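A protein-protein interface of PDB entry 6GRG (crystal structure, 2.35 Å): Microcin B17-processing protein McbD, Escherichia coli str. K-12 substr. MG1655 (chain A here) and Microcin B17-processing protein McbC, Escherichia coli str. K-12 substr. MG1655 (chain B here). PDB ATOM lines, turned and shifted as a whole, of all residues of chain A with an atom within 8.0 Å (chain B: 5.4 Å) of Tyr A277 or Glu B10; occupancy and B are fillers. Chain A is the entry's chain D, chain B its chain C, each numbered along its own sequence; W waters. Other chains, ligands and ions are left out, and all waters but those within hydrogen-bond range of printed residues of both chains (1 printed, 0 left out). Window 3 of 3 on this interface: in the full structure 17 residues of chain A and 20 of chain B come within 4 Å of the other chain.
Water W1 lies within hydrogen-bond range of the side-chain carboxylate of Glu B10 and the backbone carbonyl oxygen of Asn A271.
Tyr A277 touches just one residue of chain B: Glu B10. Glu B10 touches just one residue of chain A: Tyr A277. Printed residues of chain B within 4 Å of Pro A20: Leu B8 and Thr B12. Printed residues of chain B within 4 Å of Ser A19: Val B9. The nearest residue of chain A that does not touch Glu B10 is Gly A275 (4.6 Å).
Of the 19 printed residues of chain A, 4 touch a printed residue of chain B. Printed residues of chain A that touch a printed residue of chain B: Ser A19, Pro A20, Asn A271 and Tyr A277. Of the 9 printed residues of chain B, 5 touch a printed residue of chain A. Hydrophobic or aromatic side chains of chain B that line the printed part of chain A: Leu B8 and Val B9.
The side-chain hydroxyl of Ser B7 is in hydrogen-bond range of the side-chain amide nitrogen of Asn A271. The side-chain hydroxyl (OH) of Tyr A277 lies within hydrogen-bond range of the side-chain carboxylate (OE2) of Glu B10 (2.8 Å).
The side-chain hydroxyl of Ser B7 lies close to the backbone NH of Val B9, 3.4 Å away.
Among the printed residues, pairs that only touch across the chains: Ser A19 with Val B9, Pro A20 with Thr B12, Pro A20 with Leu B8 and Asn A271 with Val B9.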
ATOM      1  N   SER A  19       4.331  -0.240  18.199  1.00  0.00           N
ATOM      2  CA  SER A  19       3.322   0.313  17.327  1.00  0.00           C
ATOM      3  C   SER A  19       3.466   1.837  17.238  1.00  0.00           C
ATOM      4  O   SER A  19       3.533   2.514  18.247  1.00  0.00           O
ATOM      5  CB  SER A  19       1.947  -0.085  17.791  1.00  0.00           C
ATOM      6  OG  SER A  19       0.993   0.642  17.035  1.00  0.00           O
ATOM      7  N   PRO A  20       3.502   2.450  16.040  1.00  0.00           N
ATOM      8  CA  PRO A  20       3.398   3.900  15.950  1.00  0.00           C
ATOM      9  C   PRO A  20       2.091   4.332  16.619  1.00  0.00           C
ATOM     10  O   PRO A  20       1.192   3.510  16.729  1.00  0.00           O
ATOM     11  CB  PRO A  20       3.374   4.251  14.444  1.00  0.00           C
ATOM     12  CG  PRO A  20       3.583   2.942  13.701  1.00  0.00           C
ATOM     13  CD  PRO A  20       3.653   1.816  14.723  1.00  0.00           C
ATOM     14  N   GLN A  31       4.602  -5.626  20.725  1.00  0.00           N
ATOM     15  CA  GLN A  31       4.066  -6.951  20.602  1.00  0.00           C
ATOM     16  C   GLN A  31       5.047  -7.845  19.851  1.00  0.00           C
ATOM     17  O   GLN A  31       5.813  -7.365  19.081  1.00  0.00           O
ATOM     18  CB  GLN A  31       2.701  -6.871  19.922  1.00  0.00           C
ATOM     19  CG  GLN A  31       2.361  -8.095  19.098  1.00  0.00           C
ATOM     20  CD  GLN A  31       1.107  -7.873  18.296  1.00  0.00           C
ATOM     21  OE1 GLN A  31       1.158  -7.780  17.075  1.00  0.00           O
ATOM     22  NE2 GLN A  31      -0.004  -7.741  18.992  1.00  0.00           N
ATOM     23  N   CYS A 268      -6.437  -4.383  21.908  1.00  0.00           N
ATOM     24  CA  CYS A 268      -6.199  -5.640  21.211  1.00  0.00           C
ATOM     25  C   CYS A 268      -7.499  -6.189  20.635  1.00  0.00           C
ATOM     26  O   CYS A 268      -7.594  -6.432  19.450  1.00  0.00           O
ATOM     27  CB  CYS A 268      -5.559  -6.688  22.101  1.00  0.00           C
ATOM     28  SG  CYS A 268      -3.834  -6.265  22.403  1.00  0.00           S
ATOM     29  N   LEU A 269      -8.507  -6.335  21.479  1.00  0.00           N
ATOM     30  CA  LEU A 269      -9.822  -6.774  21.021  1.00  0.00           C
ATOM     31  C   LEU A 269     -10.364  -5.792  19.969  1.00  0.00           C
ATOM     32  O   LEU A 269     -10.929  -6.228  18.969  1.00  0.00           O
ATOM     33  CB  LEU A 269     -10.773  -6.887  22.218  1.00  0.00           C
ATOM     34  CG  LEU A 269     -12.145  -7.500  21.923  1.00  0.00           C
ATOM     35  CD1 LEU A 269     -12.032  -8.684  20.974  1.00  0.00           C
ATOM     36  CD2 LEU A 269     -12.843  -7.921  23.213  1.00  0.00           C
ATOM     37  N   HIS A 270     -10.199  -4.477  20.185  1.00  0.00           N
ATOM     38  CA  HIS A 270     -10.795  -3.501  19.269  1.00  0.00           C
ATOM     39  C   HIS A 270     -10.204  -3.743  17.883  1.00  0.00           C
ATOM     40  O   HIS A 270     -10.949  -3.782  16.882  1.00  0.00           O
ATOM     41  CB  HIS A 270     -10.611  -2.062  19.762  1.00  0.00           C
ATOM     42  CG  HIS A 270     -11.126  -1.035  18.816  1.00  0.00           C
ATOM     43  ND1 HIS A 270     -12.459  -0.643  18.797  1.00  0.00           N
ATOM     44  CD2 HIS A 270     -10.505  -0.330  17.841  1.00  0.00           C
ATOM     45  CE1 HIS A 270     -12.623   0.285  17.866  1.00  0.00           C
ATOM     46  NE2 HIS A 270     -11.444   0.477  17.246  1.00  0.00           N
ATOM     47  N   ASN A 271      -8.890  -3.991  17.858  1.00  0.00           N
ATOM     48  CA  ASN A 271      -8.122  -4.175  16.610  1.00  0.00           C
ATOM     49  C   ASN A 271      -8.503  -5.498  15.919  1.00  0.00           C
ATOM     50  O   ASN A 271      -8.651  -5.556  14.686  1.00  0.00           O
ATOM     51  CB  ASN A 271      -6.613  -4.028  16.867  1.00  0.00           C
ATOM     52  CG  ASN A 271      -6.226  -2.572  17.011  1.00  0.00           C
ATOM     53  OD1 ASN A 271      -6.974  -1.700  16.557  1.00  0.00           O
ATOM     54  ND2 ASN A 271      -5.064  -2.297  17.596  1.00  0.00           N
ATOM     55  N   PHE A 272      -8.642  -6.563  16.715  1.00  0.00           N
ATOM     56  CA  PHE A 272      -9.209  -7.822  16.232  1.00  0.00           C
ATOM     57  C   PHE A 272     -10.531  -7.559  15.492  1.00  0.00           C
ATOM     58  O   PHE A 272     -10.723  -7.964  14.350  1.00  0.00           O
ATOM     59  CB  PHE A 272      -9.426  -8.786  17.404  1.00  0.00           C
ATOM     60  CG  PHE A 272      -9.717 -10.202  16.988  1.00  0.00           C
ATOM     61  CD1 PHE A 272     -11.006 -10.588  16.655  1.00  0.00           C
ATOM     62  CD2 PHE A 272      -8.694 -11.131  16.899  1.00  0.00           C
ATOM     63  CE1 PHE A 272     -11.271 -11.888  16.254  1.00  0.00           C
ATOM     64  CE2 PHE A 272      -8.959 -12.429  16.491  1.00  0.00           C
ATOM     65  CZ  PHE A 272     -10.246 -12.805  16.170  1.00  0.00           C
ATOM     66  N   LEU A 273     -11.436  -6.837  16.151  1.00  0.00           N
ATOM     67  CA  LEU A 273     -12.789  -6.634  15.648  1.00  0.00           C
ATOM     68  C   LEU A 273     -12.807  -5.749  14.391  1.00  0.00           C
ATOM     69  O   LEU A 273     -13.565  -6.040  13.460  1.00  0.00           O
ATOM     70  CB  LEU A 273     -13.646  -6.038  16.769  1.00  0.00           C
ATOM     71  CG  LEU A 273     -13.881  -6.968  17.954  1.00  0.00           C
ATOM     72  CD1 LEU A 273     -14.392  -6.182  19.137  1.00  0.00           C
ATOM     73  CD2 LEU A 273     -14.841  -8.076  17.590  1.00  0.00           C
ATOM     74  N   ILE A 274     -12.012  -4.672  14.348  1.00  0.00           N
ATOM     75  CA  ILE A 274     -12.018  -3.813  13.138  1.00  0.00           C
ATOM     76  C   ILE A 274     -11.156  -4.466  12.047  1.00  0.00           C
ATOM     77  O   ILE A 274     -11.403  -4.264  10.897  1.00  0.00           O
ATOM     78  CB  ILE A 274     -11.608  -2.346  13.415  1.00  0.00           C
ATOM     79  CG1 ILE A 274     -10.176  -2.209  13.940  1.00  0.00           C
ATOM     80  CG2 ILE A 274     -12.614  -1.662  14.333  1.00  0.00           C
ATOM     81  CD1 ILE A 274      -9.658  -0.790  13.916  1.00  0.00           C
ATOM     82  N   GLY A 275     -10.168  -5.278  12.437  1.00  0.00           N
ATOM     83  CA  GLY A 275      -9.337  -6.051  11.493  1.00  0.00           C
ATOM     84  C   GLY A 275     -10.125  -7.044  10.633  1.00  0.00           C
ATOM     85  O   GLY A 275      -9.644  -7.489   9.622  1.00  0.00           O
ATOM     86  N   GLY A 276     -11.341  -7.413  11.037  1.00  0.00           N
ATOM     87  CA  GLY A 276     -12.168  -8.354  10.274  1.00  0.00           C
ATOM     88  C   GLY A 276     -11.851  -9.801  10.628  1.00  0.00           C
ATOM     89  O   GLY A 276     -12.568 -10.698  10.231  1.00  0.00           O
ATOM     90  N   TYR A 277     -10.801 -10.010  11.430  1.00  0.00           N
ATOM     91  CA  TYR A 277     -10.313 -11.331  11.822  1.00  0.00           C
ATOM     92  C   TYR A 277     -11.476 -12.222  12.301  1.00  0.00           C
ATOM     93  O   TYR A 277     -12.428 -11.765  12.945  1.00  0.00           O
ATOM     94  CB  TYR A 277      -9.215 -11.193  12.883  1.00  0.00           C
ATOM     95  CG  TYR A 277      -7.974 -10.474  12.409  1.00  0.00           C
ATOM     96  CD1 TYR A 277      -6.941 -11.154  11.783  1.00  0.00           C
ATOM     97  CD2 TYR A 277      -7.834  -9.104  12.567  1.00  0.00           C
ATOM     98  CE1 TYR A 277      -5.801 -10.497  11.342  1.00  0.00           C
ATOM     99  CE2 TYR A 277      -6.704  -8.430  12.125  1.00  0.00           C
ATOM    100  CZ  TYR A 277      -5.679  -9.128  11.510  1.00  0.00           C
ATOM    101  OH  TYR A 277      -4.560  -8.469  11.076  1.00  0.00           O
ATOM    102  N   THR A 278     -11.343 -13.514  11.982  1.00  0.00           N
ATOM    103  CA  THR A 278     -12.334 -14.575  12.162  1.00  0.00           C
ATOM    104  C   THR A 278     -12.150 -15.290  13.514  1.00  0.00           C
ATOM    105  O   THR A 278     -11.108 -15.219  14.130  1.00  0.00           O
ATOM    106  CB  THR A 278     -12.149 -15.598  11.035  1.00  0.00           C
ATOM    107  OG1 THR A 278     -10.811 -16.091  11.151  1.00  0.00           O
ATOM    108  CG2 THR A 278     -12.347 -15.022   9.649  1.00  0.00           C
ATOM    109  N   ASP A 279     -13.153 -16.069  13.929  1.00  0.00           N
ATOM    110  CA  ASP A 279     -13.048 -16.934  15.135  1.00  0.00           C
ATOM    111  C   ASP A 279     -11.902 -17.966  15.003  1.00  0.00           C
ATOM    112  O   ASP A 279     -11.290 -18.328  16.011  1.00  0.00           O
ATOM    113  CB  ASP A 279     -14.395 -17.599  15.457  1.00  0.00           C
ATOM    114  CG  ASP A 279     -15.277 -16.804  16.414  1.00  0.00           C
ATOM    115  OD1 ASP A 279     -16.521 -16.976  16.350  1.00  0.00           O
ATOM    116  OD2 ASP A 279     -14.721 -16.031  17.238  1.00  0.00           O
ATOM    117  N   ASP A 280     -11.595 -18.425  13.779  1.00  0.00           N
ATOM    118  CA  ASP A 280     -10.539 -19.409  13.534  1.00  0.00           C
ATOM    119  C   ASP A 280      -9.188 -18.792  13.906  1.00  0.00           C
ATOM    120  O   ASP A 280      -8.199 -19.508  14.073  1.00  0.00           O
ATOM    121  CB  ASP A 280     -10.541 -19.924  12.090  1.00  0.00           C
ATOM    122  N   ASP A 281      -9.158 -17.461  14.041  1.00  0.00           N
ATOM    123  CA  ASP A 281      -7.971 -16.741  14.476  1.00  0.00           C
ATOM    124  C   ASP A 281      -7.772 -16.900  15.990  1.00  0.00           C
ATOM    125  O   ASP A 281      -6.663 -16.721  16.469  1.00  0.00           O
ATOM    126  CB  ASP A 281      -8.045 -15.264  14.077  1.00  0.00           C
ATOM    127  CG  ASP A 281      -7.878 -15.036  12.581  1.00  0.00           C
ATOM    128  OD1 ASP A 281      -6.786 -15.351  12.066  1.00  0.00           O
ATOM    129  OD2 ASP A 281      -8.836 -14.543  11.937  1.00  0.00           O
ATOM    130  N   ILE A 282      -8.843 -17.212  16.735  1.00  0.00           N
ATOM    131  CA  ILE A 282      -8.763 -17.377  18.196  1.00  0.00           C
ATOM    132  C   ILE A 282      -8.436 -18.840  18.523  1.00  0.00           C
ATOM    133  O   ILE A 282      -9.255 -19.735  18.222  1.00  0.00           O
ATOM    134  CB  ILE A 282     -10.063 -16.918  18.886  1.00  0.00           C
ATOM    135  CG1 ILE A 282     -10.450 -15.488  18.495  1.00  0.00           C
ATOM    136  CG2 ILE A 282      -9.936 -17.074  20.401  1.00  0.00           C
ATOM    137  CD1 ILE A 282      -9.410 -14.450  18.900  1.00  0.00           C
ATOM    138  N   MET A 291     -13.779 -12.693  24.931  1.00  0.00           N
ATOM    139  CA  MET A 291     -14.361 -12.145  23.744  1.00  0.00           C
ATOM    140  C   MET A 291     -15.889 -12.351  23.764  1.00  0.00           C
ATOM    141  O   MET A 291     -16.613 -11.504  23.294  1.00  0.00           O
ATOM    142  CB  MET A 291     -13.743 -12.817  22.517  1.00  0.00           C
ATOM    143  CG  MET A 291     -13.509 -11.884  21.358  1.00  0.00           C
ATOM    144  SD  MET A 291     -12.994 -12.771  19.863  1.00  0.00           S
ATOM    145  CE  MET A 291     -14.590 -13.125  19.125  1.00  0.00           C
ATOM    146  N   LEU B   6      -8.233   2.630  10.641  1.00  0.00           N
ATOM    147  CA  LEU B   6      -7.081   1.780  10.466  1.00  0.00           C
ATOM    148  C   LEU B   6      -6.137   1.963  11.655  1.00  0.00           C
ATOM    149  O   LEU B   6      -5.824   3.077  12.069  1.00  0.00           O
ATOM    150  CB  LEU B   6      -6.384   2.128   9.151  1.00  0.00           C
ATOM    151  CG  LEU B   6      -5.019   1.488   8.924  1.00  0.00           C
ATOM    152  CD1 LEU B   6      -5.151  -0.008   8.647  1.00  0.00           C
ATOM    153  CD2 LEU B   6      -4.312   2.175   7.771  1.00  0.00           C
ATOM    154  N   SER B   7      -5.690   0.820  12.171  1.00  0.00           N
ATOM    155  CA  SER B   7      -4.776   0.720  13.271  1.00  0.00           C
ATOM    156  C   SER B   7      -3.341   0.724  12.746  1.00  0.00           C
ATOM    157  O   SER B   7      -2.998  -0.075  11.892  1.00  0.00           O
ATOM    158  CB  SER B   7      -5.067  -0.541  14.031  1.00  0.00           C
ATOM    159  OG  SER B   7      -4.148  -0.728  15.086  1.00  0.00           O
ATOM    160  N   LEU B   8      -2.498   1.598  13.286  1.00  0.00           N
ATOM    161  CA  LEU B   8      -1.112   1.665  12.846  1.00  0.00           C
ATOM    162  C   LEU B   8      -0.357   0.362  13.159  1.00  0.00           C
ATOM    163  O   LEU B   8       0.707   0.135  12.603  1.00  0.00           O
ATOM    164  CB  LEU B   8      -0.465   2.891  13.491  1.00  0.00           C
ATOM    165  CG  LEU B   8      -0.955   4.191  12.855  1.00  0.00           C
ATOM    166  CD1 LEU B   8      -0.349   5.416  13.525  1.00  0.00           C
ATOM    167  CD2 LEU B   8      -0.656   4.183  11.353  1.00  0.00           C
ATOM    168  N   VAL B   9      -0.917  -0.497  14.020  1.00  0.00           N
ATOM    169  CA  VAL B   9      -0.300  -1.790  14.332  1.00  0.00           C
ATOM    170  C   VAL B   9      -0.287  -2.651  13.068  1.00  0.00           C
ATOM    171  O   VAL B   9       0.590  -3.444  12.880  1.00  0.00           O
ATOM    172  CB  VAL B   9      -1.014  -2.561  15.465  1.00  0.00           C
ATOM    173  CG1 VAL B   9      -0.143  -3.701  15.985  1.00  0.00           C
ATOM    174  CG2 VAL B   9      -1.434  -1.678  16.636  1.00  0.00           C
ATOM    175  N   GLU B  10      -1.319  -2.537  12.237  1.00  0.00           N
ATOM    176  CA  GLU B  10      -1.375  -3.313  11.001  1.00  0.00           C
ATOM    177  C   GLU B  10      -0.265  -2.853  10.053  1.00  0.00           C
ATOM    178  O   GLU B  10       0.362  -3.648   9.389  1.00  0.00           O
ATOM    179  CB  GLU B  10      -2.744  -3.151  10.342  1.00  0.00           C
ATOM    180  CG  GLU B  10      -3.875  -3.747  11.154  1.00  0.00           C
ATOM    181  CD  GLU B  10      -4.008  -5.257  11.064  1.00  0.00           C
ATOM    182  OE1 GLU B  10      -3.375  -5.853  10.184  1.00  0.00           O
ATOM    183  OE2 GLU B  10      -4.769  -5.832  11.861  1.00  0.00           O
ATOM    184  N   VAL B  11      -0.053  -1.539  10.020  1.00  0.00           N
ATOM    185  CA  VAL B  11       0.896  -0.890   9.167  1.00  0.00           C
ATOM    186  C   VAL B  11       2.322  -1.323   9.535  1.00  0.00           C
ATOM    187  O   VAL B  11       3.102  -1.690   8.662  1.00  0.00           O
ATOM    188  CB  VAL B  11       0.741   0.643   9.237  1.00  0.00           C
ATOM    189  CG1 VAL B  11       1.887   1.352   8.541  1.00  0.00           C
ATOM    190  CG2 VAL B  11      -0.603   1.079   8.672  1.00  0.00           C
ATOM    191  N   THR B  12       2.656  -1.282  10.821  1.00  0.00           N
ATOM    192  CA  THR B  12       4.039  -1.477  11.241  1.00  0.00           C
ATOM    193  C   THR B  12       4.516  -2.901  10.925  1.00  0.00           C
ATOM    194  O   THR B  12       5.715  -3.103  10.855  1.00  0.00           O
ATOM    195  CB  THR B  12       4.271  -1.145  12.720  1.00  0.00           C
ATOM    196  OG1 THR B  12       5.680  -0.959  12.865  1.00  0.00           O
ATOM    197  CG2 THR B  12       3.756  -2.191  13.696  1.00  0.00           C
ATOM    198  N   HIS B  13       3.595  -3.851  10.698  1.00  0.00           N
ATOM    199  CA  HIS B  13       3.956  -5.233  10.395  1.00  0.00           C
ATOM    200  C   HIS B  13       4.776  -5.301   9.089  1.00  0.00           C
ATOM    201  O   HIS B  13       5.470  -6.286   8.833  1.00  0.00           O
ATOM    202  CB  HIS B  13       2.678  -6.080  10.420  1.00  0.00           C
ATOM    203  CG  HIS B  13       2.815  -7.508  10.017  1.00  0.00           C
ATOM    204  ND1 HIS B  13       3.233  -8.492  10.898  1.00  0.00           N
ATOM    205  CD2 HIS B  13       2.508  -8.142   8.856  1.00  0.00           C
ATOM    206  CE1 HIS B  13       3.216  -9.666  10.283  1.00  0.00           C
ATOM    207  NE2 HIS B  13       2.767  -9.477   9.027  1.00  0.00           N
ATOM    208  N   TYR B  14       4.719  -4.245   8.272  1.00  0.00           N
ATOM    209  CA  TYR B  14       5.403  -4.219   6.998  1.00  0.00           C
ATOM    210  C   TYR B  14       6.570  -3.229   6.990  1.00  0.00           C
ATOM    211  O   TYR B  14       7.148  -3.027   5.950  1.00  0.00           O
ATOM    212  CB  TYR B  14       4.426  -3.833   5.881  1.00  0.00           C
ATOM    213  CG  TYR B  14       3.337  -4.853   5.670  1.00  0.00           C
ATOM    214  CD1 TYR B  14       3.594  -6.044   5.013  1.00  0.00           C
ATOM    215  CD2 TYR B  14       2.063  -4.660   6.184  1.00  0.00           C
ATOM    216  CE1 TYR B  14       2.612  -7.015   4.873  1.00  0.00           C
ATOM    217  CE2 TYR B  14       1.073  -5.615   6.047  1.00  0.00           C
ATOM    218  CZ  TYR B  14       1.345  -6.795   5.383  1.00  0.00           C
ATOM    219  OH  TYR B  14       0.353  -7.720   5.220  1.00  0.00           O
HETATM  220  O   HOH W   1      -6.615  -4.077  12.933  1.00  0.00           O
